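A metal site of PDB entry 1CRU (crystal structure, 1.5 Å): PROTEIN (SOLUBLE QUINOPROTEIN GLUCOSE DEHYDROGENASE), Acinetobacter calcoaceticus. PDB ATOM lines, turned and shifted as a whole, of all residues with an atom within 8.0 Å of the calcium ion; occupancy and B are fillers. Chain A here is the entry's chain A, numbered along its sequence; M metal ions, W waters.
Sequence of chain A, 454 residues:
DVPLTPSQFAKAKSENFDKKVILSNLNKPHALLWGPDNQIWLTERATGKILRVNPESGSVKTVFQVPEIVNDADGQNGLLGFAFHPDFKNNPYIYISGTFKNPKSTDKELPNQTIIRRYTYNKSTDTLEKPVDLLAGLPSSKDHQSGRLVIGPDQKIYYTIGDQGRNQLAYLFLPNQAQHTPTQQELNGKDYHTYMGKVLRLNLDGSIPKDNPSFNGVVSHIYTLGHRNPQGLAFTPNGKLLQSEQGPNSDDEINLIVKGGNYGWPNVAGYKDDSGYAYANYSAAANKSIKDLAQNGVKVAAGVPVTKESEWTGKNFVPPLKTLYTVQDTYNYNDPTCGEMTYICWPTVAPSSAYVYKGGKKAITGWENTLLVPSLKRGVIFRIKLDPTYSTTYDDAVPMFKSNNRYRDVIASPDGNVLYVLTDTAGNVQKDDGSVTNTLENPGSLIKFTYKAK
OD1 of Asp 273 lies close to N of Ser 275 (3.1 Å).
N of Glu 309 sits at hydrogen-bond distance from OD1 of Asp 274, 3.1 Å away.
Within 4 Å of the calcium ion: Ala 269, Tyr 271, Asp 273 and Glu 309.
The nearest printed residue that does not touch the calcium ion is Gly 270 (4.2 Å).
The calcium ion is bound by the backbone carbonyl oxygen (O) of Ala 269, the side-chain carboxylate (OD1) of Asp 273, the backbone carbonyl oxygen (O) of Tyr 271, water W2, the side-chain carboxylate (OE2) of Glu 309, the side-chain carboxylate (OE1) of Glu 309 and water W1.
Water W2 bridges O of Ser 275 (2.7 Å) and OD2 of Asp 251 (2.8 Å).
Water W1 lies within hydrogen-bond range of the side-chain carboxylate (OD2) of Asp 273 (2.7 Å), the side-chain carboxylate (OD1) of Asp 251 (2.7 Å), the backbone NH (N) of Tyr 271 (3.0 Å) and the side-chain hydroxyl (OG1) of Thr 326 (3.5 Å).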
ATOM      1  N   SER A 250       6.577   7.909  28.689  1.00  0.00           N
ATOM      2  CA  SER A 250       5.466   7.938  27.740  1.00  0.00           C
ATOM      3  C   SER A 250       4.462   6.851  28.114  1.00  0.00           C
ATOM      4  O   SER A 250       4.730   6.037  28.981  1.00  0.00           O
ATOM      5  CB  SER A 250       5.999   7.630  26.330  1.00  0.00           C
ATOM      6  OG  SER A 250       6.481   6.304  26.260  1.00  0.00           O
ATOM      7  N   ASP A 251       3.354   6.840  27.377  1.00  0.00           N
ATOM      8  CA  ASP A 251       2.457   5.696  27.381  1.00  0.00           C
ATOM      9  C   ASP A 251       1.889   5.303  28.743  1.00  0.00           C
ATOM     10  O   ASP A 251       1.874   4.115  29.093  1.00  0.00           O
ATOM     11  CB  ASP A 251       3.159   4.500  26.719  1.00  0.00           C
ATOM     12  CG  ASP A 251       3.432   4.735  25.240  1.00  0.00           C
ATOM     13  OD1 ASP A 251       2.453   4.678  24.465  1.00  0.00           O
ATOM     14  OD2 ASP A 251       4.588   4.970  24.845  1.00  0.00           O
ATOM     15  N   GLU A 253      -1.418   4.390  30.580  1.00  0.00           N
ATOM     16  CA  GLU A 253      -2.448   3.619  29.890  1.00  0.00           C
ATOM     17  C   GLU A 253      -3.776   3.583  30.613  1.00  0.00           C
ATOM     18  O   GLU A 253      -3.838   3.585  31.838  1.00  0.00           O
ATOM     19  CB  GLU A 253      -1.999   2.144  29.818  1.00  0.00           C
ATOM     20  CG  GLU A 253      -0.823   1.912  28.894  1.00  0.00           C
ATOM     21  CD  GLU A 253      -0.317   0.494  28.911  1.00  0.00           C
ATOM     22  OE1 GLU A 253      -0.678  -0.296  29.821  1.00  0.00           O
ATOM     23  OE2 GLU A 253       0.471   0.141  28.002  1.00  0.00           O
ATOM     24  N   ASN A 267       8.466  -5.086  28.261  1.00  0.00           N
ATOM     25  CA  ASN A 267       8.846  -5.221  26.845  1.00  0.00           C
ATOM     26  C   ASN A 267       8.061  -4.294  25.943  1.00  0.00           C
ATOM     27  O   ASN A 267       8.607  -3.878  24.904  1.00  0.00           O
ATOM     28  CB  ASN A 267       8.631  -6.676  26.409  1.00  0.00           C
ATOM     29  CG  ASN A 267       9.618  -7.547  27.167  1.00  0.00           C
ATOM     30  OD1 ASN A 267       9.346  -8.002  28.278  1.00  0.00           O
ATOM     31  ND2 ASN A 267      10.766  -7.782  26.534  1.00  0.00           N
ATOM     32  N   VAL A 268       6.843  -3.932  26.337  1.00  0.00           N
ATOM     33  CA  VAL A 268       6.032  -3.030  25.552  1.00  0.00           C
ATOM     34  C   VAL A 268       5.386  -1.951  26.410  1.00  0.00           C
ATOM     35  O   VAL A 268       4.726  -2.274  27.396  1.00  0.00           O
ATOM     36  CB  VAL A 268       4.908  -3.804  24.805  1.00  0.00           C
ATOM     37  CG1 VAL A 268       4.116  -2.870  23.901  1.00  0.00           C
ATOM     38  CG2 VAL A 268       5.486  -4.971  24.027  1.00  0.00           C
ATOM     39  N   ALA A 269       5.570  -0.695  26.033  1.00  0.00           N
ATOM     40  CA  ALA A 269       4.915   0.433  26.687  1.00  0.00           C
ATOM     41  C   ALA A 269       3.791   0.896  25.758  1.00  0.00           C
ATOM     42  O   ALA A 269       4.085   1.298  24.616  1.00  0.00           O
ATOM     43  CB  ALA A 269       5.894   1.566  26.938  1.00  0.00           C
ATOM     44  N   GLY A 270       2.540   0.856  26.194  1.00  0.00           N
ATOM     45  CA  GLY A 270       1.420   1.264  25.354  1.00  0.00           C
ATOM     46  C   GLY A 270       1.182   0.200  24.276  1.00  0.00           C
ATOM     47  O   GLY A 270       1.177  -1.006  24.513  1.00  0.00           O
ATOM     48  N   TYR A 271       0.952   0.718  23.058  1.00  0.00           N
ATOM     49  CA  TYR A 271       0.783  -0.196  21.934  1.00  0.00           C
ATOM     50  C   TYR A 271       2.107  -0.835  21.542  1.00  0.00           C
ATOM     51  O   TYR A 271       3.182  -0.288  21.827  1.00  0.00           O
ATOM     52  CB  TYR A 271       0.276   0.602  20.729  1.00  0.00           C
ATOM     53  CG  TYR A 271      -0.992   1.369  21.000  1.00  0.00           C
ATOM     54  CD1 TYR A 271      -0.983   2.736  21.178  1.00  0.00           C
ATOM     55  CD2 TYR A 271      -2.227   0.710  21.092  1.00  0.00           C
ATOM     56  CE1 TYR A 271      -2.141   3.456  21.434  1.00  0.00           C
ATOM     57  CE2 TYR A 271      -3.378   1.406  21.343  1.00  0.00           C
ATOM     58  CZ  TYR A 271      -3.344   2.770  21.508  1.00  0.00           C
ATOM     59  OH  TYR A 271      -4.494   3.483  21.765  1.00  0.00           O
ATOM     60  N   LYS A 272       2.051  -1.974  20.869  1.00  0.00           N
ATOM     61  CA  LYS A 272       3.262  -2.604  20.345  1.00  0.00           C
ATOM     62  C   LYS A 272       3.570  -1.926  19.013  1.00  0.00           C
ATOM     63  O   LYS A 272       3.171  -2.407  17.943  1.00  0.00           O
ATOM     64  CB  LYS A 272       3.100  -4.112  20.170  1.00  0.00           C
ATOM     65  CG  LYS A 272       4.404  -4.821  19.845  1.00  0.00           C
ATOM     66  CD  LYS A 272       4.165  -6.247  19.383  1.00  0.00           C
ATOM     67  CE  LYS A 272       3.758  -7.151  20.535  1.00  0.00           C
ATOM     68  NZ  LYS A 272       3.746  -8.570  20.109  1.00  0.00           N
ATOM     69  N   ASP A 273       4.180  -0.748  19.087  1.00  0.00           N
ATOM     70  CA  ASP A 273       4.350   0.130  17.939  1.00  0.00           C
ATOM     71  C   ASP A 273       5.783   0.544  17.635  1.00  0.00           C
ATOM     72  O   ASP A 273       5.987   1.215  16.607  1.00  0.00           O
ATOM     73  CB  ASP A 273       3.470   1.367  18.132  1.00  0.00           C
ATOM     74  CG  ASP A 273       3.689   2.166  19.409  1.00  0.00           C
ATOM     75  OD1 ASP A 273       4.651   1.868  20.136  1.00  0.00           O
ATOM     76  OD2 ASP A 273       2.874   3.077  19.668  1.00  0.00           O
ATOM     77  N   ASP A 274       6.743   0.159  18.462  1.00  0.00           N
ATOM     78  CA  ASP A 274       8.127   0.588  18.309  1.00  0.00           C
ATOM     79  C   ASP A 274       8.217   2.099  18.199  1.00  0.00           C
ATOM     80  O   ASP A 274       9.064   2.634  17.467  1.00  0.00           O
ATOM     81  CB  ASP A 274       8.780  -0.060  17.088  1.00  0.00           C
ATOM     82  CG  ASP A 274       9.024  -1.544  17.221  1.00  0.00           C
ATOM     83  OD1 ASP A 274       8.758  -2.128  18.296  1.00  0.00           O
ATOM     84  OD2 ASP A 274       9.487  -2.180  16.249  1.00  0.00           O
ATOM     85  N   SER A 275       7.349   2.829  18.891  1.00  0.00           N
ATOM     86  CA  SER A 275       7.308   4.278  18.778  1.00  0.00           C
ATOM     87  C   SER A 275       7.524   5.008  20.098  1.00  0.00           C
ATOM     88  O   SER A 275       6.647   5.019  20.956  1.00  0.00           O
ATOM     89  CB  SER A 275       5.965   4.690  18.163  1.00  0.00           C
ATOM     90  OG  SER A 275       5.915   6.062  17.864  1.00  0.00           O
ATOM     91  N   GLY A 276       8.691   5.626  20.220  1.00  0.00           N
ATOM     92  CA  GLY A 276       8.999   6.443  21.382  1.00  0.00           C
ATOM     93  C   GLY A 276       9.487   5.686  22.599  1.00  0.00           C
ATOM     94  O   GLY A 276       9.789   6.347  23.608  1.00  0.00           O
ATOM     95  N   TYR A 277       9.574   4.379  22.566  1.00  0.00           N
ATOM     96  CA  TYR A 277      10.034   3.548  23.662  1.00  0.00           C
ATOM     97  C   TYR A 277      10.734   2.309  23.129  1.00  0.00           C
ATOM     98  O   TYR A 277      10.349   1.787  22.070  1.00  0.00           O
ATOM     99  CB  TYR A 277       8.861   3.074  24.544  1.00  0.00           C
ATOM    100  CG  TYR A 277       9.250   2.083  25.625  1.00  0.00           C
ATOM    101  CD1 TYR A 277       9.805   2.539  26.825  1.00  0.00           C
ATOM    102  CD2 TYR A 277       9.096   0.716  25.481  1.00  0.00           C
ATOM    103  CE1 TYR A 277      10.182   1.652  27.813  1.00  0.00           C
ATOM    104  CE2 TYR A 277       9.465  -0.180  26.462  1.00  0.00           C
ATOM    105  CZ  TYR A 277      10.003   0.298  27.637  1.00  0.00           C
ATOM    106  OH  TYR A 277      10.370  -0.601  28.609  1.00  0.00           O
ATOM    107  N   ALA A 278      11.731   1.817  23.845  1.00  0.00           N
ATOM    108  CA  ALA A 278      12.323   0.508  23.604  1.00  0.00           C
ATOM    109  C   ALA A 278      12.755  -0.041  24.978  1.00  0.00           C
ATOM    110  O   ALA A 278      12.931   0.763  25.881  1.00  0.00           O
ATOM    111  CB  ALA A 278      13.482   0.523  22.619  1.00  0.00           C
ATOM    112  N   ASN A 296      13.913   7.062  27.491  1.00  0.00           N
ATOM    113  CA  ASN A 296      12.871   6.079  27.227  1.00  0.00           C
ATOM    114  C   ASN A 296      13.346   4.913  26.381  1.00  0.00           C
ATOM    115  O   ASN A 296      12.526   4.197  25.789  1.00  0.00           O
ATOM    116  CB  ASN A 296      11.650   6.806  26.645  1.00  0.00           C
ATOM    117  CG  ASN A 296      10.361   6.277  27.247  1.00  0.00           C
ATOM    118  OD1 ASN A 296      10.333   5.922  28.436  1.00  0.00           O
ATOM    119  ND2 ASN A 296       9.282   6.219  26.477  1.00  0.00           N
ATOM    120  N   GLU A 309       9.919  -3.273  20.895  1.00  0.00           N
ATOM    121  CA  GLU A 309       8.638  -3.880  21.285  1.00  0.00           C
ATOM    122  C   GLU A 309       8.276  -5.037  20.350  1.00  0.00           C
ATOM    123  O   GLU A 309       7.764  -6.058  20.793  1.00  0.00           O
ATOM    124  CB  GLU A 309       7.564  -2.797  21.270  1.00  0.00           C
ATOM    125  CG  GLU A 309       7.876  -1.720  22.312  1.00  0.00           C
ATOM    126  CD  GLU A 309       6.832  -0.641  22.356  1.00  0.00           C
ATOM    127  OE1 GLU A 309       6.269  -0.285  21.283  1.00  0.00           O
ATOM    128  OE2 GLU A 309       6.513  -0.088  23.436  1.00  0.00           O
ATOM    129  N   PHE A 317      -0.670 -10.872  24.678  1.00  0.00           N
ATOM    130  CA  PHE A 317      -0.495  -9.441  24.811  1.00  0.00           C
ATOM    131  C   PHE A 317      -1.782  -8.683  24.537  1.00  0.00           C
ATOM    132  O   PHE A 317      -2.406  -8.816  23.484  1.00  0.00           O
ATOM    133  CB  PHE A 317       0.630  -8.938  23.885  1.00  0.00           C
ATOM    134  CG  PHE A 317       0.695  -7.435  23.897  1.00  0.00           C
ATOM    135  CD1 PHE A 317       1.028  -6.751  25.053  1.00  0.00           C
ATOM    136  CD2 PHE A 317       0.405  -6.694  22.759  1.00  0.00           C
ATOM    137  CE1 PHE A 317       1.070  -5.372  25.075  1.00  0.00           C
ATOM    138  CE2 PHE A 317       0.446  -5.317  22.771  1.00  0.00           C
ATOM    139  CZ  PHE A 317       0.787  -4.638  23.938  1.00  0.00           C
ATOM    140  N   PRO A 320      -3.489  -1.315  25.362  1.00  0.00           N
ATOM    141  CA  PRO A 320      -4.330  -0.395  26.099  1.00  0.00           C
ATOM    142  C   PRO A 320      -5.493   0.118  25.287  1.00  0.00           C
ATOM    143  O   PRO A 320      -5.416   0.185  24.050  1.00  0.00           O
ATOM    144  CB  PRO A 320      -3.358   0.744  26.444  1.00  0.00           C
ATOM    145  CG  PRO A 320      -2.398   0.734  25.287  1.00  0.00           C
ATOM    146  CD  PRO A 320      -2.186  -0.729  24.975  1.00  0.00           C
ATOM    147  N   THR A 323      -3.786   5.581  25.341  1.00  0.00           N
ATOM    148  CA  THR A 323      -2.478   5.938  25.867  1.00  0.00           C
ATOM    149  C   THR A 323      -2.421   7.448  26.100  1.00  0.00           C
ATOM    150  O   THR A 323      -2.952   8.253  25.341  1.00  0.00           O
ATOM    151  CB  THR A 323      -1.303   5.551  24.969  1.00  0.00           C
ATOM    152  OG1 THR A 323      -1.507   6.142  23.672  1.00  0.00           O
ATOM    153  CG2 THR A 323      -1.142   4.049  24.846  1.00  0.00           C
ATOM    154  N   TYR A 325       0.734   9.556  27.015  1.00  0.00           N
ATOM    155  CA  TYR A 325       0.438   9.649  25.587  1.00  0.00           C
ATOM    156  C   TYR A 325       1.464   8.889  24.762  1.00  0.00           C
ATOM    157  O   TYR A 325       2.524   8.454  25.218  1.00  0.00           O
ATOM    158  CB  TYR A 325       0.546  11.123  25.178  1.00  0.00           C
ATOM    159  CG  TYR A 325      -0.412  12.038  25.903  1.00  0.00           C
ATOM    160  CD1 TYR A 325       0.037  12.855  26.958  1.00  0.00           C
ATOM    161  CD2 TYR A 325      -1.750  12.107  25.571  1.00  0.00           C
ATOM    162  CE1 TYR A 325      -0.848  13.691  27.610  1.00  0.00           C
ATOM    163  CE2 TYR A 325      -2.637  12.940  26.214  1.00  0.00           C
ATOM    164  CZ  TYR A 325      -2.181  13.734  27.264  1.00  0.00           C
ATOM    165  OH  TYR A 325      -3.070  14.564  27.898  1.00  0.00           O
ATOM    166  N   THR A 326       1.201   8.715  23.451  1.00  0.00           N
ATOM    167  CA  THR A 326       2.162   8.081  22.556  1.00  0.00           C
ATOM    168  C   THR A 326       2.833   9.131  21.656  1.00  0.00           C
ATOM    169  O   THR A 326       2.141  10.025  21.181  1.00  0.00           O
ATOM    170  CB  THR A 326       1.475   7.017  21.678  1.00  0.00           C
ATOM    171  OG1 THR A 326       0.953   6.017  22.561  1.00  0.00           O
ATOM    172  CG2 THR A 326       2.454   6.349  20.716  1.00  0.00           C
ATOM    173  N   VAL A 327       4.131   8.985  21.510  1.00  0.00           N
ATOM    174  CA  VAL A 327       4.908   9.908  20.673  1.00  0.00           C
ATOM    175  C   VAL A 327       5.762   9.084  19.716  1.00  0.00           C
ATOM    176  O   VAL A 327       5.949   7.872  19.850  1.00  0.00           O
ATOM    177  CB  VAL A 327       5.792  10.864  21.500  1.00  0.00           C
ATOM    178  CG1 VAL A 327       4.921  11.746  22.379  1.00  0.00           C
ATOM    179  CG2 VAL A 327       6.822  10.119  22.329  1.00  0.00           C
HETATM  180 CA    CA M   1       4.738   1.366  22.429  1.00  0.00          CA
HETATM  181  O   HOH W   1       2.711   3.003  22.349  1.00  0.00           O
HETATM  182  O   HOH W   2       5.938   3.325  22.987  1.00  0.00           O
